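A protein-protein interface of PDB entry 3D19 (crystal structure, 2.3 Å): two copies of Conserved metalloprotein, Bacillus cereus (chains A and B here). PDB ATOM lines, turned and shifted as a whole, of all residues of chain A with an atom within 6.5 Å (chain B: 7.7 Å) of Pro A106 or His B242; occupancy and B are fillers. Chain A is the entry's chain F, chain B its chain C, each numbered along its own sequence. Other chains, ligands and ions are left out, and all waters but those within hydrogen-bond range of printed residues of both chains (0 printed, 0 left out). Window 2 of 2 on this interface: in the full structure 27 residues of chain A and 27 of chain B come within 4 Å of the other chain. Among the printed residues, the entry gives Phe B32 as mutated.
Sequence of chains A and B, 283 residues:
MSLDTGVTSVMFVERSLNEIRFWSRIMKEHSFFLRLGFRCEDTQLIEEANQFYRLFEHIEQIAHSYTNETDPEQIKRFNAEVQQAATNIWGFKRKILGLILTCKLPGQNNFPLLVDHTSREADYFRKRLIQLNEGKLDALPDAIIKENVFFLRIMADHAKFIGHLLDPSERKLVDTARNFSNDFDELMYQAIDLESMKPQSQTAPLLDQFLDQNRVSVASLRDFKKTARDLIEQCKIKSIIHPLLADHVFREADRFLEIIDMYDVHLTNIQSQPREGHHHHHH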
ATOM      1  N   ARG A  39     -10.942  13.758  22.852  1.00  0.00           N
ATOM      2  CA  ARG A  39     -11.222  13.009  24.083  1.00  0.00           C
ATOM      3  C   ARG A  39     -10.169  13.461  25.071  1.00  0.00           C
ATOM      4  O   ARG A  39      -9.095  13.917  24.666  1.00  0.00           O
ATOM      5  CB  ARG A  39     -11.121  11.508  23.874  1.00  0.00           C
ATOM      6  CG  ARG A  39     -11.989  11.060  22.758  1.00  0.00           C
ATOM      7  CD  ARG A  39     -11.606   9.759  22.161  1.00  0.00           C
ATOM      8  NE  ARG A  39     -10.181   9.490  22.042  1.00  0.00           N
ATOM      9  CZ  ARG A  39      -9.717   8.242  21.980  1.00  0.00           C
ATOM     10  NH1 ARG A  39     -10.578   7.221  22.009  1.00  0.00           N
ATOM     11  NH2 ARG A  39      -8.424   7.992  21.906  1.00  0.00           N
ATOM     12  N   GLU A  41      -8.203  12.004  27.190  1.00  0.00           N
ATOM     13  CA  GLU A  41      -6.953  11.281  27.111  1.00  0.00           C
ATOM     14  C   GLU A  41      -6.072  11.570  25.880  1.00  0.00           C
ATOM     15  O   GLU A  41      -4.920  11.186  25.852  1.00  0.00           O
ATOM     16  CB  GLU A  41      -7.269   9.810  27.137  1.00  0.00           C
ATOM     17  CG  GLU A  41      -7.811   9.347  25.820  1.00  0.00           C
ATOM     18  CD  GLU A  41      -8.942   8.368  25.995  1.00  0.00           C
ATOM     19  OE1 GLU A  41     -10.069   8.840  26.327  1.00  0.00           O
ATOM     20  OE2 GLU A  41      -8.679   7.145  25.793  1.00  0.00           O
ATOM     21  N   CYS A 103     -11.413   5.618  12.572  1.00  0.00           N
ATOM     22  CA  CYS A 103     -11.936   5.159  13.862  1.00  0.00           C
ATOM     23  C   CYS A 103     -10.878   4.892  14.902  1.00  0.00           C
ATOM     24  O   CYS A 103     -11.000   3.943  15.669  1.00  0.00           O
ATOM     25  CB  CYS A 103     -12.728   3.884  13.713  1.00  0.00           C
ATOM     26  SG  CYS A 103     -14.177   4.038  12.708  1.00  0.00           S
ATOM     27  N   LYS A 104      -9.847   5.730  14.908  1.00  0.00           N
ATOM     28  CA  LYS A 104      -8.825   5.660  15.910  1.00  0.00           C
ATOM     29  C   LYS A 104      -9.193   6.445  17.213  1.00  0.00           C
ATOM     30  O   LYS A 104      -8.498   6.328  18.225  1.00  0.00           O
ATOM     31  CB  LYS A 104      -7.493   6.106  15.300  1.00  0.00           C
ATOM     32  CG  LYS A 104      -6.559   4.935  14.901  1.00  0.00           C
ATOM     33  CD  LYS A 104      -6.515   4.641  13.409  1.00  0.00           C
ATOM     34  CE  LYS A 104      -5.063   4.291  12.901  1.00  0.00           C
ATOM     35  NZ  LYS A 104      -4.063   5.475  12.730  1.00  0.00           N
ATOM     36  N   LEU A 105     -10.300   7.194  17.199  1.00  0.00           N
ATOM     37  CA  LEU A 105     -10.687   8.039  18.328  1.00  0.00           C
ATOM     38  C   LEU A 105     -12.192   7.923  18.739  1.00  0.00           C
ATOM     39  O   LEU A 105     -12.927   8.944  18.745  1.00  0.00           O
ATOM     40  CB  LEU A 105     -10.353   9.512  18.034  1.00  0.00           C
ATOM     41  CG  LEU A 105      -8.960   9.773  17.453  1.00  0.00           C
ATOM     42  CD1 LEU A 105      -8.878  11.163  16.867  1.00  0.00           C
ATOM     43  CD2 LEU A 105      -7.889   9.562  18.495  1.00  0.00           C
ATOM     44  N   PRO A 106     -12.643   6.684  19.068  1.00  0.00           N
ATOM     45  CA  PRO A 106     -13.993   6.434  19.554  1.00  0.00           C
ATOM     46  C   PRO A 106     -14.282   7.286  20.786  1.00  0.00           C
ATOM     47  O   PRO A 106     -13.479   7.317  21.706  1.00  0.00           O
ATOM     48  CB  PRO A 106     -13.959   4.936  19.941  1.00  0.00           C
ATOM     49  CG  PRO A 106     -12.506   4.585  20.065  1.00  0.00           C
ATOM     50  CD  PRO A 106     -11.875   5.430  18.964  1.00  0.00           C
ATOM     51  N   GLY A 107     -15.424   7.962  20.815  1.00  0.00           N
ATOM     52  CA  GLY A 107     -15.722   8.891  21.896  1.00  0.00           C
ATOM     53  C   GLY A 107     -15.528  10.360  21.506  1.00  0.00           C
ATOM     54  O   GLY A 107     -15.988  11.273  22.209  1.00  0.00           O
ATOM     55  N   GLN A 108     -14.848  10.608  20.391  1.00  0.00           N
ATOM     56  CA  GLN A 108     -14.482  11.988  20.039  1.00  0.00           C
ATOM     57  C   GLN A 108     -15.704  12.625  19.378  1.00  0.00           C
ATOM     58  O   GLN A 108     -16.615  11.891  18.916  1.00  0.00           O
ATOM     59  CB  GLN A 108     -13.227  12.027  19.171  1.00  0.00           C
ATOM     60  CG  GLN A 108     -13.416  11.696  17.700  1.00  0.00           C
ATOM     61  CD  GLN A 108     -13.885  12.887  16.898  1.00  0.00           C
ATOM     62  OE1 GLN A 108     -13.421  14.029  17.099  1.00  0.00           O
ATOM     63  NE2 GLN A 108     -14.801  12.642  15.964  1.00  0.00           N
ATOM     64  N   PHE B  32     -21.275   6.231  30.946  1.00  0.00           N
ATOM     65  CA  PHE B  32     -20.215   6.352  30.035  1.00  0.00           C
ATOM     66  C   PHE B  32     -20.482   7.448  29.009  1.00  0.00           C
ATOM     67  O   PHE B  32     -19.634   8.296  28.804  1.00  0.00           O
ATOM     68  CB  PHE B  32     -19.988   4.989  29.385  1.00  0.00           C
ATOM     69  CG  PHE B  32     -19.035   5.003  28.256  1.00  0.00           C
ATOM     70  CD1 PHE B  32     -17.681   5.183  28.472  1.00  0.00           C
ATOM     71  CD2 PHE B  32     -19.482   4.795  26.961  1.00  0.00           C
ATOM     72  CE1 PHE B  32     -16.790   5.180  27.395  1.00  0.00           C
ATOM     73  CE2 PHE B  32     -18.592   4.806  25.886  1.00  0.00           C
ATOM     74  CZ  PHE B  32     -17.255   4.986  26.109  1.00  0.00           C
ATOM     75  N   PHE B  33     -21.660   7.488  28.389  1.00  0.00           N
ATOM     76  CA  PHE B  33     -21.937   8.529  27.383  1.00  0.00           C
ATOM     77  C   PHE B  33     -21.925   9.925  27.992  1.00  0.00           C
ATOM     78  O   PHE B  33     -21.408  10.867  27.431  1.00  0.00           O
ATOM     79  CB  PHE B  33     -23.295   8.295  26.728  1.00  0.00           C
ATOM     80  CG  PHE B  33     -23.478   6.896  26.207  1.00  0.00           C
ATOM     81  CD1 PHE B  33     -22.524   6.321  25.403  1.00  0.00           C
ATOM     82  CD2 PHE B  33     -24.613   6.159  26.527  1.00  0.00           C
ATOM     83  CE1 PHE B  33     -22.690   5.018  24.932  1.00  0.00           C
ATOM     84  CE2 PHE B  33     -24.781   4.866  26.050  1.00  0.00           C
ATOM     85  CZ  PHE B  33     -23.825   4.298  25.263  1.00  0.00           C
ATOM     86  N   LEU B  36     -18.297  11.158  28.377  1.00  0.00           N
ATOM     87  CA  LEU B  36     -17.814  11.609  27.046  1.00  0.00           C
ATOM     88  C   LEU B  36     -18.259  13.027  26.627  1.00  0.00           C
ATOM     89  O   LEU B  36     -17.597  13.679  25.824  1.00  0.00           O
ATOM     90  CB  LEU B  36     -18.272  10.650  25.952  1.00  0.00           C
ATOM     91  CG  LEU B  36     -17.798   9.198  25.984  1.00  0.00           C
ATOM     92  CD1 LEU B  36     -18.184   8.617  24.670  1.00  0.00           C
ATOM     93  CD2 LEU B  36     -16.277   9.062  26.191  1.00  0.00           C
ATOM     94  N   LEU B 165     -26.006  13.233  15.410  1.00  0.00           N
ATOM     95  CA  LEU B 165     -24.685  12.694  15.603  1.00  0.00           C
ATOM     96  C   LEU B 165     -24.052  12.156  14.297  1.00  0.00           C
ATOM     97  O   LEU B 165     -22.844  11.983  14.208  1.00  0.00           O
ATOM     98  CB  LEU B 165     -24.737  11.629  16.672  1.00  0.00           C
ATOM     99  CG  LEU B 165     -24.564  12.108  18.139  1.00  0.00           C
ATOM    100  CD1 LEU B 165     -24.600  13.615  18.243  1.00  0.00           C
ATOM    101  CD2 LEU B 165     -25.489  11.427  19.202  1.00  0.00           C
ATOM    102  N   ARG B 229     -25.370   0.319  13.483  1.00  0.00           N
ATOM    103  CA  ARG B 229     -24.384  -0.186  14.442  1.00  0.00           C
ATOM    104  C   ARG B 229     -23.258  -0.897  13.680  1.00  0.00           C
ATOM    105  O   ARG B 229     -22.057  -0.668  13.956  1.00  0.00           O
ATOM    106  CB  ARG B 229     -25.022  -1.149  15.448  1.00  0.00           C
ATOM    107  CG  ARG B 229     -24.076  -1.651  16.475  1.00  0.00           C
ATOM    108  CD  ARG B 229     -24.595  -2.914  17.146  1.00  0.00           C
ATOM    109  NE  ARG B 229     -24.898  -3.925  16.134  1.00  0.00           N
ATOM    110  CZ  ARG B 229     -25.478  -5.107  16.374  1.00  0.00           C
ATOM    111  NH1 ARG B 229     -25.828  -5.431  17.617  1.00  0.00           N
ATOM    112  NH2 ARG B 229     -25.713  -5.968  15.370  1.00  0.00           N
ATOM    113  N   ILE B 232     -20.995   1.422  11.694  1.00  0.00           N
ATOM    114  CA  ILE B 232     -20.126   2.208  12.536  1.00  0.00           C
ATOM    115  C   ILE B 232     -18.978   1.348  13.080  1.00  0.00           C
ATOM    116  O   ILE B 232     -17.807   1.777  13.159  1.00  0.00           O
ATOM    117  CB  ILE B 232     -20.891   2.814  13.718  1.00  0.00           C
ATOM    118  CG1 ILE B 232     -21.719   4.011  13.269  1.00  0.00           C
ATOM    119  CG2 ILE B 232     -19.911   3.275  14.751  1.00  0.00           C
ATOM    120  CD1 ILE B 232     -22.819   4.306  14.222  1.00  0.00           C
ATOM    121  N   GLU B 233     -19.321   0.126  13.464  1.00  0.00           N
ATOM    122  CA  GLU B 233     -18.336  -0.825  13.970  1.00  0.00           C
ATOM    123  C   GLU B 233     -17.289  -1.119  12.916  1.00  0.00           C
ATOM    124  O   GLU B 233     -16.143  -1.366  13.254  1.00  0.00           O
ATOM    125  CB  GLU B 233     -18.976  -2.167  14.341  1.00  0.00           C
ATOM    126  CG  GLU B 233     -19.774  -2.165  15.617  1.00  0.00           C
ATOM    127  CD  GLU B 233     -20.441  -3.506  15.828  1.00  0.00           C
ATOM    128  OE1 GLU B 233     -20.498  -4.309  14.855  1.00  0.00           O
ATOM    129  OE2 GLU B 233     -20.912  -3.764  16.960  1.00  0.00           O
ATOM    130  N   SER B 239     -19.496   9.636  11.403  1.00  0.00           N
ATOM    131  CA  SER B 239     -20.359  10.058  12.470  1.00  0.00           C
ATOM    132  C   SER B 239     -19.575  10.361  13.720  1.00  0.00           C
ATOM    133  O   SER B 239     -18.398   9.933  13.867  1.00  0.00           O
ATOM    134  CB  SER B 239     -21.388   8.946  12.777  1.00  0.00           C
ATOM    135  OG  SER B 239     -20.816   7.878  13.527  1.00  0.00           O
ATOM    136  N   ILE B 240     -20.217  11.074  14.653  1.00  0.00           N
ATOM    137  CA  ILE B 240     -19.664  11.076  15.998  1.00  0.00           C
ATOM    138  C   ILE B 240     -20.480  10.151  16.935  1.00  0.00           C
ATOM    139  O   ILE B 240     -20.733  10.528  18.052  1.00  0.00           O
ATOM    140  CB  ILE B 240     -19.437  12.492  16.607  1.00  0.00           C
ATOM    141  CG1 ILE B 240     -20.743  13.242  16.709  1.00  0.00           C
ATOM    142  CG2 ILE B 240     -18.369  13.303  15.739  1.00  0.00           C
ATOM    143  CD1 ILE B 240     -20.669  14.497  17.540  1.00  0.00           C
ATOM    144  N   ILE B 241     -20.872   8.965  16.475  1.00  0.00           N
ATOM    145  CA  ILE B 241     -21.685   8.028  17.284  1.00  0.00           C
ATOM    146  C   ILE B 241     -20.761   6.925  17.768  1.00  0.00           C
ATOM    147  O   ILE B 241     -20.305   6.127  16.985  1.00  0.00           O
ATOM    148  CB  ILE B 241     -22.809   7.385  16.439  1.00  0.00           C
ATOM    149  CG1 ILE B 241     -23.834   8.424  16.045  1.00  0.00           C
ATOM    150  CG2 ILE B 241     -23.583   6.293  17.233  1.00  0.00           C
ATOM    151  CD1 ILE B 241     -24.808   7.983  14.938  1.00  0.00           C
ATOM    152  N   HIS B 242     -20.409   6.906  19.036  1.00  0.00           N
ATOM    153  CA  HIS B 242     -19.631   5.760  19.547  1.00  0.00           C
ATOM    154  C   HIS B 242     -20.382   4.474  19.144  1.00  0.00           C
ATOM    155  O   HIS B 242     -21.609   4.451  19.193  1.00  0.00           O
ATOM    156  CB  HIS B 242     -19.523   5.867  21.066  1.00  0.00           C
ATOM    157  CG  HIS B 242     -18.510   4.958  21.682  1.00  0.00           C
ATOM    158  ND1 HIS B 242     -18.733   3.608  21.860  1.00  0.00           N
ATOM    159  CD2 HIS B 242     -17.284   5.212  22.209  1.00  0.00           C
ATOM    160  CE1 HIS B 242     -17.680   3.061  22.451  1.00  0.00           C
ATOM    161  NE2 HIS B 242     -16.794   4.015  22.689  1.00  0.00           N
ATOM    162  N   PRO B 243     -19.668   3.431  18.692  1.00  0.00           N
ATOM    163  CA  PRO B 243     -20.318   2.152  18.410  1.00  0.00           C
ATOM    164  C   PRO B 243     -21.257   1.695  19.497  1.00  0.00           C
ATOM    165  O   PRO B 243     -22.281   1.095  19.206  1.00  0.00           O
ATOM    166  CB  PRO B 243     -19.156   1.155  18.348  1.00  0.00           C
ATOM    167  CG  PRO B 243     -17.968   1.935  18.096  1.00  0.00           C
ATOM    168  CD  PRO B 243     -18.200   3.318  18.626  1.00  0.00           C
ATOM    169  N   LEU B 244     -20.922   1.950  20.747  1.00  0.00           N
ATOM    170  CA  LEU B 244     -21.695   1.406  21.868  1.00  0.00           C
ATOM    171  C   LEU B 244     -23.031   2.135  21.966  1.00  0.00           C
ATOM    172  O   LEU B 244     -24.025   1.576  22.459  1.00  0.00           O
ATOM    173  CB  LEU B 244     -20.894   1.557  23.166  1.00  0.00           C
ATOM    174  CG  LEU B 244     -21.433   0.981  24.495  1.00  0.00           C
ATOM    175  CD1 LEU B 244     -21.952  -0.514  24.413  1.00  0.00           C
ATOM    176  CD2 LEU B 244     -20.343   1.081  25.516  1.00  0.00           C
ATOM    177  N   LEU B 245     -23.054   3.392  21.489  1.00  0.00           N
ATOM    178  CA  LEU B 245     -24.261   4.167  21.576  1.00  0.00           C
ATOM    179  C   LEU B 245     -25.174   3.556  20.545  1.00  0.00           C
ATOM    180  O   LEU B 245     -26.378   3.394  20.787  1.00  0.00           O
ATOM    181  CB  LEU B 245     -23.974   5.638  21.299  1.00  0.00           C
ATOM    182  CG  LEU B 245     -25.090   6.666  21.137  1.00  0.00           C
ATOM    183  CD1 LEU B 245     -26.239   6.377  22.056  1.00  0.00           C
ATOM    184  CD2 LEU B 245     -24.505   8.089  21.466  1.00  0.00           C
ATOM    185  N   ALA B 246     -24.603   3.165  19.416  1.00  0.00           N
ATOM    186  CA  ALA B 246     -25.383   2.465  18.409  1.00  0.00           C
ATOM    187  C   ALA B 246     -26.032   1.150  18.898  1.00  0.00           C
ATOM    188  O   ALA B 246     -27.199   0.907  18.616  1.00  0.00           O
ATOM    189  CB  ALA B 246     -24.549   2.198  17.164  1.00  0.00           C
ATOM    190  N   ASP B 247     -25.276   0.300  19.590  1.00  0.00           N
ATOM    191  CA  ASP B 247     -25.807  -1.006  20.047  1.00  0.00           C
ATOM    192  C   ASP B 247     -26.861  -0.784  21.154  1.00  0.00           C
ATOM    193  O   ASP B 247     -27.884  -1.421  21.194  1.00  0.00           O
ATOM    194  CB  ASP B 247     -24.668  -1.889  20.559  1.00  0.00           C
ATOM    195  CG  ASP B 247     -25.156  -3.278  21.077  1.00  0.00           C
ATOM    196  OD1 ASP B 247     -25.724  -4.099  20.309  1.00  0.00           O
ATOM    197  OD2 ASP B 247     -24.922  -3.577  22.267  1.00  0.00           O
ATOM    198  N   HIS B 248     -26.588   0.157  22.028  1.00  0.00           N
ATOM    199  CA  HIS B 248     -27.473   0.591  23.080  1.00  0.00           C
ATOM    200  C   HIS B 248     -28.894   0.907  22.573  1.00  0.00           C
ATOM    201  O   HIS B 248     -29.854   0.252  22.966  1.00  0.00           O
ATOM    202  CB  HIS B 248     -26.815   1.810  23.702  1.00  0.00           C
ATOM    203  CG  HIS B 248     -27.577   2.447  24.811  1.00  0.00           C
ATOM    204  ND1 HIS B 248     -27.298   2.202  26.138  1.00  0.00           N
ATOM    205  CD2 HIS B 248     -28.555   3.387  24.801  1.00  0.00           C
ATOM    206  CE1 HIS B 248     -28.081   2.944  26.894  1.00  0.00           C
ATOM    207  NE2 HIS B 248     -28.860   3.666  26.111  1.00  0.00           N
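No position is printed for both chains.
Of the 4 pairs that touch across the chains among the printed residues, none has its exchanged pair printed and touching as well.
The backbone carbonyl oxygen (O) of Leu B165 is in hydrogen-bond range of the backbone NH (N) of Ile B240.
N of Leu B244 sits at hydrogen-bond distance from ND1 of His B242, 3.0 Å away.
The guanidinium group of Arg A39 is in hydrogen-bond range of the backbone carbonyl oxygen of Pro A106.
C of Pro A106 touches CD2 of His B242 (3.9 Å).
Gly A107 touches Leu B36 (CA to CD1, 3.7 Å).
Gly A107 touches His B242 (N to CD2, 3.6 Å).
Gln A108 touches Ile B240.
His B242 touches just these residues of chain A: Pro A106 and Gly A107.
Of the printed residues of chain A, Ile B240 touches Gln A108 (3.6 Å).
Of the printed residues of chain B, Gly A107 touches Leu B36 (3.7 Å) and His B242 (3.6 Å).
Ser B239 touches none of the printed residues of chain A.
The nearest residue of chain A that does not touch His B242 is Gln A108 (6.2 Å).
Of the 17 printed residues of chain B, 3 touch a printed residue of chain A.
Printed residues of chain B that touch a printed residue of chain A: Leu B36, Ile B240 and His B242.
Hydrophobic or aromatic side chains of chain B within 4 Å of the printed part of chain A: Leu B36, Ile B240 and His B242.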
